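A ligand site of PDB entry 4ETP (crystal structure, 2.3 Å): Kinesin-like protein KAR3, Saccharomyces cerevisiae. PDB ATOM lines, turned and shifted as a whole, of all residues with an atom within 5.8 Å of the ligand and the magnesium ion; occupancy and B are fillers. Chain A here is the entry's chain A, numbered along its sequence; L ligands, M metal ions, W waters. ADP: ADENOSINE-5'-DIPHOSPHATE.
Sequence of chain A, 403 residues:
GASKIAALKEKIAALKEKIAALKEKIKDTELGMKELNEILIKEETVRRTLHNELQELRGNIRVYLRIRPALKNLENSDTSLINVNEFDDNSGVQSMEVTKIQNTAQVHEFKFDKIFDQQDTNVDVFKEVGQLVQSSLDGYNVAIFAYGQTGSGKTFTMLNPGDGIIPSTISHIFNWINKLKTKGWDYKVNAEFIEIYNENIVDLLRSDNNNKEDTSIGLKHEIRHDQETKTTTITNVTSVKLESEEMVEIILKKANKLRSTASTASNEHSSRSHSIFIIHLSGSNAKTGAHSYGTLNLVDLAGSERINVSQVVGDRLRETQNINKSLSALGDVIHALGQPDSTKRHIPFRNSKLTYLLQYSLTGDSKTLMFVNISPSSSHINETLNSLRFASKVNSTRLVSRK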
ATOM      1  N   ARG A  66      16.974   7.498  26.029  1.00  0.00           N
ATOM      2  CA  ARG A  66      18.374   7.097  25.912  1.00  0.00           C
ATOM      3  C   ARG A  66      19.321   8.276  25.966  1.00  0.00           C
ATOM      4  O   ARG A  66      19.306   9.151  25.102  1.00  0.00           O
ATOM      5  CB  ARG A  66      18.637   6.282  24.643  1.00  0.00           C
ATOM      6  CG  ARG A  66      20.081   5.800  24.614  1.00  0.00           C
ATOM      7  CD  ARG A  66      20.461   5.013  23.382  1.00  0.00           C
ATOM      8  NE  ARG A  66      21.713   4.299  23.613  1.00  0.00           N
ATOM      9  CZ  ARG A  66      22.289   3.483  22.743  1.00  0.00           C
ATOM     10  NH1 ARG A  66      21.738   3.282  21.544  1.00  0.00           N
ATOM     11  NH2 ARG A  66      23.420   2.876  23.064  1.00  0.00           N
ATOM     12  N   ILE A  67      20.158   8.287  27.001  1.00  0.00           N
ATOM     13  CA  ILE A  67      21.203   9.282  27.147  1.00  0.00           C
ATOM     14  C   ILE A  67      22.484   8.711  26.578  1.00  0.00           C
ATOM     15  O   ILE A  67      23.011   7.730  27.104  1.00  0.00           O
ATOM     16  CB  ILE A  67      21.428   9.669  28.616  1.00  0.00           C
ATOM     17  CG1 ILE A  67      20.082   9.946  29.326  1.00  0.00           C
ATOM     18  CG2 ILE A  67      22.363  10.865  28.715  1.00  0.00           C
ATOM     19  CD1 ILE A  67      20.188  10.067  30.829  1.00  0.00           C
ATOM     20  N   ARG A  68      22.968   9.295  25.496  1.00  0.00           N
ATOM     21  CA  ARG A  68      24.205   8.859  24.875  1.00  0.00           C
ATOM     22  C   ARG A  68      25.404   9.326  25.727  1.00  0.00           C
ATOM     23  O   ARG A  68      25.255  10.224  26.552  1.00  0.00           O
ATOM     24  CB  ARG A  68      24.316   9.402  23.444  1.00  0.00           C
ATOM     25  CG  ARG A  68      24.327  10.917  23.322  1.00  0.00           C
ATOM     26  CD  ARG A  68      25.187  11.363  22.158  1.00  0.00           C
ATOM     27  NE  ARG A  68      25.046  12.791  21.861  1.00  0.00           N
ATOM     28  CZ  ARG A  68      25.647  13.773  22.534  1.00  0.00           C
ATOM     29  NH1 ARG A  68      25.444  15.032  22.166  1.00  0.00           N
ATOM     30  NH2 ARG A  68      26.456  13.500  23.552  1.00  0.00           N
ATOM     31  N   PRO A  69      26.582   8.710  25.521  1.00  0.00           N
ATOM     32  CA  PRO A  69      27.794   9.200  26.172  1.00  0.00           C
ATOM     33  C   PRO A  69      28.092  10.648  25.778  1.00  0.00           C
ATOM     34  O   PRO A  69      27.773  11.068  24.673  1.00  0.00           O
ATOM     35  CB  PRO A  69      28.896   8.293  25.608  1.00  0.00           C
ATOM     36  CG  PRO A  69      28.190   7.031  25.235  1.00  0.00           C
ATOM     37  CD  PRO A  69      26.820   7.447  24.796  1.00  0.00           C
ATOM     38  N   LEU A  71      30.303  13.801  24.553  1.00  0.00           N
ATOM     39  CA  LEU A  71      31.286  13.924  23.481  1.00  0.00           C
ATOM     40  C   LEU A  71      32.266  15.062  23.757  1.00  0.00           C
ATOM     41  O   LEU A  71      31.888  16.236  23.728  1.00  0.00           O
ATOM     42  CB  LEU A  71      30.583  14.153  22.130  1.00  0.00           C
ATOM     43  CG  LEU A  71      29.559  13.121  21.639  1.00  0.00           C
ATOM     44  CD1 LEU A  71      28.681  13.733  20.561  1.00  0.00           C
ATOM     45  CD2 LEU A  71      30.230  11.854  21.129  1.00  0.00           C
ATOM     46  N   ASP A 120      24.977   2.493  28.933  1.00  0.00           N
ATOM     47  CA  ASP A 120      24.151   1.487  28.265  1.00  0.00           C
ATOM     48  C   ASP A 120      24.431   1.431  26.760  1.00  0.00           C
ATOM     49  O   ASP A 120      24.257   2.416  26.036  1.00  0.00           O
ATOM     50  CB  ASP A 120      22.659   1.700  28.555  1.00  0.00           C
ATOM     51  CG  ASP A 120      22.322   1.428  30.011  1.00  0.00           C
ATOM     52  OD1 ASP A 120      22.691   0.353  30.522  1.00  0.00           O
ATOM     53  OD2 ASP A 120      21.665   2.286  30.642  1.00  0.00           O
ATOM     54  N   ASN A 122      24.367  -0.384  22.734  1.00  0.00           N
ATOM     55  CA  ASN A 122      23.394  -0.862  21.770  1.00  0.00           C
ATOM     56  C   ASN A 122      22.947  -2.297  22.053  1.00  0.00           C
ATOM     57  O   ASN A 122      21.784  -2.641  21.825  1.00  0.00           O
ATOM     58  CB  ASN A 122      23.962  -0.741  20.359  1.00  0.00           C
ATOM     59  CG  ASN A 122      23.943   0.687  19.833  1.00  0.00           C
ATOM     60  OD1 ASN A 122      23.598   1.626  20.553  1.00  0.00           O
ATOM     61  ND2 ASN A 122      24.286   0.846  18.555  1.00  0.00           N
ATOM     62  N   GLY A 148      14.624  12.932  18.698  1.00  0.00           N
ATOM     63  CA  GLY A 148      15.548  13.809  19.425  1.00  0.00           C
ATOM     64  C   GLY A 148      16.273  14.770  18.505  1.00  0.00           C
ATOM     65  O   GLY A 148      16.202  14.647  17.286  1.00  0.00           O
ATOM     66  N   GLN A 149      16.997  15.712  19.104  1.00  0.00           N
ATOM     67  CA  GLN A 149      17.714  16.734  18.327  1.00  0.00           C
ATOM     68  C   GLN A 149      18.829  16.110  17.476  1.00  0.00           C
ATOM     69  O   GLN A 149      19.360  15.047  17.828  1.00  0.00           O
ATOM     70  CB  GLN A 149      18.270  17.831  19.237  1.00  0.00           C
ATOM     71  CG  GLN A 149      19.444  17.400  20.111  1.00  0.00           C
ATOM     72  CD  GLN A 149      20.076  18.550  20.878  1.00  0.00           C
ATOM     73  OE1 GLN A 149      20.371  19.617  20.311  1.00  0.00           O
ATOM     74  NE2 GLN A 149      20.291  18.348  22.169  1.00  0.00           N
ATOM     75  N   THR A 150      19.171  16.768  16.376  1.00  0.00           N
ATOM     76  CA  THR A 150      20.353  16.390  15.592  1.00  0.00           C
ATOM     77  C   THR A 150      21.548  16.364  16.548  1.00  0.00           C
ATOM     78  O   THR A 150      21.752  17.308  17.318  1.00  0.00           O
ATOM     79  CB  THR A 150      20.599  17.373  14.435  1.00  0.00           C
ATOM     80  OG1 THR A 150      19.437  17.417  13.601  1.00  0.00           O
ATOM     81  CG2 THR A 150      21.816  16.955  13.599  1.00  0.00           C
ATOM     82  N   GLY A 151      22.305  15.270  16.504  1.00  0.00           N
ATOM     83  CA  GLY A 151      23.456  15.084  17.385  1.00  0.00           C
ATOM     84  C   GLY A 151      23.183  14.270  18.635  1.00  0.00           C
ATOM     85  O   GLY A 151      24.114  13.962  19.374  1.00  0.00           O
ATOM     86  N   SER A 152      21.920  13.913  18.886  1.00  0.00           N
ATOM     87  CA  SER A 152      21.550  13.220  20.131  1.00  0.00           C
ATOM     88  C   SER A 152      21.744  11.695  20.080  1.00  0.00           C
ATOM     89  O   SER A 152      21.767  11.038  21.125  1.00  0.00           O
ATOM     90  CB  SER A 152      20.121  13.571  20.547  1.00  0.00           C
ATOM     91  OG  SER A 152      19.165  13.054  19.641  1.00  0.00           O
ATOM     92  N   GLY A 153      21.870  11.145  18.871  1.00  0.00           N
ATOM     93  CA  GLY A 153      22.199   9.738  18.694  1.00  0.00           C
ATOM     94  C   GLY A 153      21.128   8.848  18.074  1.00  0.00           C
ATOM     95  O   GLY A 153      21.152   7.635  18.253  1.00  0.00           O
ATOM     96  N   LYS A 154      20.206   9.446  17.327  1.00  0.00           N
ATOM     97  CA  LYS A 154      19.132   8.685  16.671  1.00  0.00           C
ATOM     98  C   LYS A 154      19.667   7.667  15.675  1.00  0.00           C
ATOM     99  O   LYS A 154      19.283   6.499  15.714  1.00  0.00           O
ATOM    100  CB  LYS A 154      18.130   9.612  15.978  1.00  0.00           C
ATOM    101  CG  LYS A 154      17.370  10.543  16.919  1.00  0.00           C
ATOM    102  CD  LYS A 154      16.463  11.505  16.148  1.00  0.00           C
ATOM    103  CE  LYS A 154      17.217  12.363  15.151  1.00  0.00           C
ATOM    104  NZ  LYS A 154      18.191  13.310  15.773  1.00  0.00           N
ATOM    105  N   THR A 155      20.554   8.122  14.790  1.00  0.00           N
ATOM    106  CA  THR A 155      21.102   7.263  13.741  1.00  0.00           C
ATOM    107  C   THR A 155      22.021   6.173  14.316  1.00  0.00           C
ATOM    108  O   THR A 155      21.987   5.034  13.859  1.00  0.00           O
ATOM    109  CB  THR A 155      21.809   8.095  12.648  1.00  0.00           C
ATOM    110  OG1 THR A 155      20.923   9.137  12.201  1.00  0.00           O
ATOM    111  CG2 THR A 155      22.208   7.236  11.448  1.00  0.00           C
ATOM    112  N   PHE A 156      22.822   6.533  15.317  1.00  0.00           N
ATOM    113  CA  PHE A 156      23.666   5.556  16.002  1.00  0.00           C
ATOM    114  C   PHE A 156      22.811   4.441  16.607  1.00  0.00           C
ATOM    115  O   PHE A 156      23.101   3.265  16.427  1.00  0.00           O
ATOM    116  CB  PHE A 156      24.520   6.236  17.084  1.00  0.00           C
ATOM    117  CG  PHE A 156      25.497   5.312  17.776  1.00  0.00           C
ATOM    118  CD1 PHE A 156      26.835   5.276  17.366  1.00  0.00           C
ATOM    119  CD2 PHE A 156      25.091   4.498  18.823  1.00  0.00           C
ATOM    120  CE1 PHE A 156      27.744   4.445  17.996  1.00  0.00           C
ATOM    121  CE2 PHE A 156      26.007   3.655  19.457  1.00  0.00           C
ATOM    122  CZ  PHE A 156      27.329   3.626  19.044  1.00  0.00           C
ATOM    123  N   THR A 157      21.755   4.839  17.317  1.00  0.00           N
ATOM    124  CA  THR A 157      20.837   3.901  17.952  1.00  0.00           C
ATOM    125  C   THR A 157      20.239   2.954  16.902  1.00  0.00           C
ATOM    126  O   THR A 157      20.163   1.750  17.122  1.00  0.00           O
ATOM    127  CB  THR A 157      19.732   4.659  18.729  1.00  0.00           C
ATOM    128  OG1 THR A 157      20.310   5.317  19.860  1.00  0.00           O
ATOM    129  CG2 THR A 157      18.633   3.715  19.199  1.00  0.00           C
ATOM    130  N   ARG A 259      22.897   9.568   8.836  1.00  0.00           N
ATOM    131  CA  ARG A 259      23.201   8.955   7.545  1.00  0.00           C
ATOM    132  C   ARG A 259      24.206   9.787   6.754  1.00  0.00           C
ATOM    133  O   ARG A 259      25.390   9.867   7.115  1.00  0.00           O
ATOM    134  CB  ARG A 259      21.921   8.768   6.727  1.00  0.00           C
ATOM    135  CG  ARG A 259      21.007   7.637   7.186  1.00  0.00           C
ATOM    136  CD  ARG A 259      19.870   7.408   6.205  1.00  0.00           C
ATOM    137  NE  ARG A 259      18.882   8.486   6.236  1.00  0.00           N
ATOM    138  CZ  ARG A 259      18.291   9.027   5.170  1.00  0.00           C
ATOM    139  NH1 ARG A 259      18.609   8.605   3.943  1.00  0.00           N
ATOM    140  NH2 ARG A 259      17.407  10.004   5.327  1.00  0.00           N
ATOM    141  N   SER A 270      19.516  14.321   5.584  1.00  0.00           N
ATOM    142  CA  SER A 270      19.082  13.213   6.437  1.00  0.00           C
ATOM    143  C   SER A 270      18.599  13.672   7.821  1.00  0.00           C
ATOM    144  O   SER A 270      17.626  13.137   8.336  1.00  0.00           O
ATOM    145  CB  SER A 270      20.193  12.175   6.595  1.00  0.00           C
ATOM    146  OG  SER A 270      20.385  11.453   5.392  1.00  0.00           O
ATOM    147  N   SER A 271      19.277  14.672   8.392  1.00  0.00           N
ATOM    148  CA  SER A 271      18.893  15.240   9.682  1.00  0.00           C
ATOM    149  C   SER A 271      17.617  16.091   9.599  1.00  0.00           C
ATOM    150  O   SER A 271      17.036  16.437  10.639  1.00  0.00           O
ATOM    151  CB  SER A 271      20.030  16.075  10.254  1.00  0.00           C
ATOM    152  OG  SER A 271      20.097  17.345   9.618  1.00  0.00           O
ATOM    153  N   ASP A 300      13.903   6.535  11.743  1.00  0.00           N
ATOM    154  CA  ASP A 300      14.905   7.508  12.194  1.00  0.00           C
ATOM    155  C   ASP A 300      14.323   8.875  11.852  1.00  0.00           C
ATOM    156  O   ASP A 300      14.320   9.301  10.690  1.00  0.00           O
ATOM    157  CB  ASP A 300      16.238   7.254  11.475  1.00  0.00           C
ATOM    158  CG  ASP A 300      17.386   8.154  11.967  1.00  0.00           C
ATOM    159  OD1 ASP A 300      17.166   9.077  12.783  1.00  0.00           O
ATOM    160  OD2 ASP A 300      18.534   7.923  11.522  1.00  0.00           O
ATOM    161  N   ASN A 373      16.122  10.123  22.279  1.00  0.00           N
ATOM    162  CA  ASN A 373      17.558  10.276  22.463  1.00  0.00           C
ATOM    163  C   ASN A 373      17.893  11.665  22.983  1.00  0.00           C
ATOM    164  O   ASN A 373      17.374  12.655  22.469  1.00  0.00           O
ATOM    165  CB  ASN A 373      18.281  10.032  21.138  1.00  0.00           C
ATOM    166  CG  ASN A 373      18.080   8.620  20.605  1.00  0.00           C
ATOM    167  OD1 ASN A 373      17.139   8.366  19.850  1.00  0.00           O
ATOM    168  ND2 ASN A 373      18.944   7.699  21.019  1.00  0.00           N
HETATM  169  PB  ADP L   1      21.545  11.995  15.300  1.00  0.00           P
HETATM  170  O1B ADP L   1      20.526  12.067  16.410  1.00  0.00           O
HETATM  171  O2B ADP L   1      21.317  10.892  14.299  1.00  0.00           O
HETATM  172  O3B ADP L   1      21.878  13.333  14.697  1.00  0.00           O
HETATM  173  PA  ADP L   1      24.054  10.618  15.528  1.00  0.00           P
HETATM  174  O1A ADP L   1      23.613   9.172  15.518  1.00  0.00           O
HETATM  175  O2A ADP L   1      24.602  11.246  14.269  1.00  0.00           O
HETATM  176  O3A ADP L   1      22.870  11.554  16.089  1.00  0.00           O
HETATM  177  O5' ADP L   1      25.128  10.788  16.715  1.00  0.00           O
HETATM  178  C5' ADP L   1      25.931  11.971  16.870  1.00  0.00           C
HETATM  179  C4' ADP L   1      27.321  11.579  17.368  1.00  0.00           C
HETATM  180  O4' ADP L   1      27.215  10.933  18.639  1.00  0.00           O
HETATM  181  C3' ADP L   1      28.009  10.571  16.445  1.00  0.00           C
HETATM  182  O3' ADP L   1      29.405  10.847  16.409  1.00  0.00           O
HETATM  183  C2' ADP L   1      27.789   9.232  17.109  1.00  0.00           C
HETATM  184  O2' ADP L   1      28.861   8.331  16.811  1.00  0.00           O
HETATM  185  C1' ADP L   1      27.739   9.601  18.581  1.00  0.00           C
HETATM  186  N9  ADP L   1      26.834   8.729  19.364  1.00  0.00           N
HETATM  187  C8  ADP L   1      25.484   8.794  19.355  1.00  0.00           C
HETATM  188  N7  ADP L   1      24.943   7.865  20.185  1.00  0.00           N
HETATM  189  C5  ADP L   1      25.965   7.193  20.749  1.00  0.00           C
HETATM  190  C6  ADP L   1      26.105   6.082  21.708  1.00  0.00           C
HETATM  191  N6  ADP L   1      25.014   5.500  22.259  1.00  0.00           N
HETATM  192  N1  ADP L   1      27.362   5.673  22.031  1.00  0.00           N
HETATM  193  C2  ADP L   1      28.463   6.239  21.493  1.00  0.00           C
HETATM  194  N3  ADP L   1      28.395   7.254  20.604  1.00  0.00           N
HETATM  195  C4  ADP L   1      27.210   7.762  20.204  1.00  0.00           C
HETATM  196 MG    MG M   1      20.966  11.218  12.249  1.00  0.00          MG
HETATM  197  O   HOH W   1      31.266   8.362  20.542  1.00  0.00           O
HETATM  198  O   HOH W   2      23.143  11.018  12.031  1.00  0.00           O
HETATM  199  O   HOH W   3      24.374  14.168  13.879  1.00  0.00           O
HETATM  200  O   HOH W   4      28.198   7.460  14.372  1.00  0.00           O
HETATM  201  O   HOH W   5      27.014  11.494  12.810  1.00  0.00           O
HETATM  202  O   HOH W   6      22.443   6.794  21.215  1.00  0.00           O
HETATM  203  O   HOH W   7      27.452   3.276  23.326  1.00  0.00           O
HETATM  204  O   HOH W   8      25.469   7.853  13.580  1.00  0.00           O
HETATM  205  O   HOH W   9      18.876  11.010  12.343  1.00  0.00           O
HETATM  206  O   HOH W  10      20.967  11.087  10.162  1.00  0.00           O
HETATM  207  O   HOH W  11      28.631  13.445  14.375  1.00  0.00           O
HETATM  208  O   HOH W  12      20.845  13.194  12.211  1.00  0.00           O
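The magnesium ion is bound by water W12 (2.0 Å), OG1 of Thr 155 (2.1 Å), water W10 (2.1 Å), water W9 (2.1 Å), O2B of the ligand (2.1 Å) and water W2 (2.2 Å).
The magnesium ion has six donor atoms within binding distance.
The backbone NH of Thr 155 lies within hydrogen-bond range of an oxygen (O1A) of the ligand (3.3 Å).
The backbone NH (N) of Gly 151 sits at hydrogen-bond distance from an oxygen (O3B) of the ligand, at 2.7 Å.
The backbone NH (N) of Lys 154 lies within hydrogen-bond range of an oxygen (O1B) of the ligand, 2.8 Å away.
NZ of Lys 154 is in salt-bridge range of O1B of the ligand, at 2.7 Å.
The backbone NH of Phe 156 is in hydrogen-bond range of an oxygen (O1A) of the ligand (2.8 Å).
N of Gly 153 sits at hydrogen-bond distance from O1B of the ligand (3.0 Å).
The backbone NH of Ser 152 lies within hydrogen-bond range of an oxygen (O1B) of the ligand (3.4 Å).
The side-chain carboxylate (OD2) of Asp 300 sits close to the side-chain hydroxyl (OG1) of Thr 155 (2.8 Å).
The side-chain amino group (NZ) of Lys 154 sits at hydrogen-bond distance from the backbone carbonyl oxygen (O) of Gln 149, 2.9 Å away.
The backbone carbonyl oxygen (O) of Gly 148 lies within hydrogen-bond range of the side-chain amino group (NZ) of Lys 154, 2.8 Å away.
O of Phe 156 sits close to ND2 of Asn 122 (3.4 Å).
NH1 of Arg 66 lies within hydrogen-bond range of OD1 of Asn 122, 2.7 Å away.
O of Asp 120 sits at hydrogen-bond distance from NH2 of Arg 66 (3.1 Å).
NH1 of Arg 66 lies within hydrogen-bond range of OG1 of Thr 157, at 3.0 Å.
The backbone carbonyl oxygen of Gln 149 is in hydrogen-bond range of the side-chain hydroxyl of Ser 152 (2.7 Å).
Water W6 lies within hydrogen-bond range of N7 of the ligand (2.9 Å), OG1 of Thr 157 (2.9 Å) and O of Gly 153 (3.3 Å).
Water W8 bridges O1A of the ligand (3.0 Å) and N of Phe 156 (3.4 Å).
The guanidinium group of Arg 66 lies close to a nitrogen (N6) of the ligand (3.2 Å).
Arg 68 touches the ligand.
Pro 69 touches the ligand.
Leu 71 touches the ligand (CD1 to O4', 3.7 Å).
O of Gln 149 touches O1B of the ligand, at 3.5 Å.
CA of Thr 150 touches O3B of the ligand, 3.5 Å away.
Of the 22 residues printed, 12 come within 4 Å of the ligand.
The nearest printed residue that does not touch the ligand is Asn 122 (4.5 Å).
The nearest printed residue that does not touch the magnesium ion is Asp 300 (4.2 Å).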
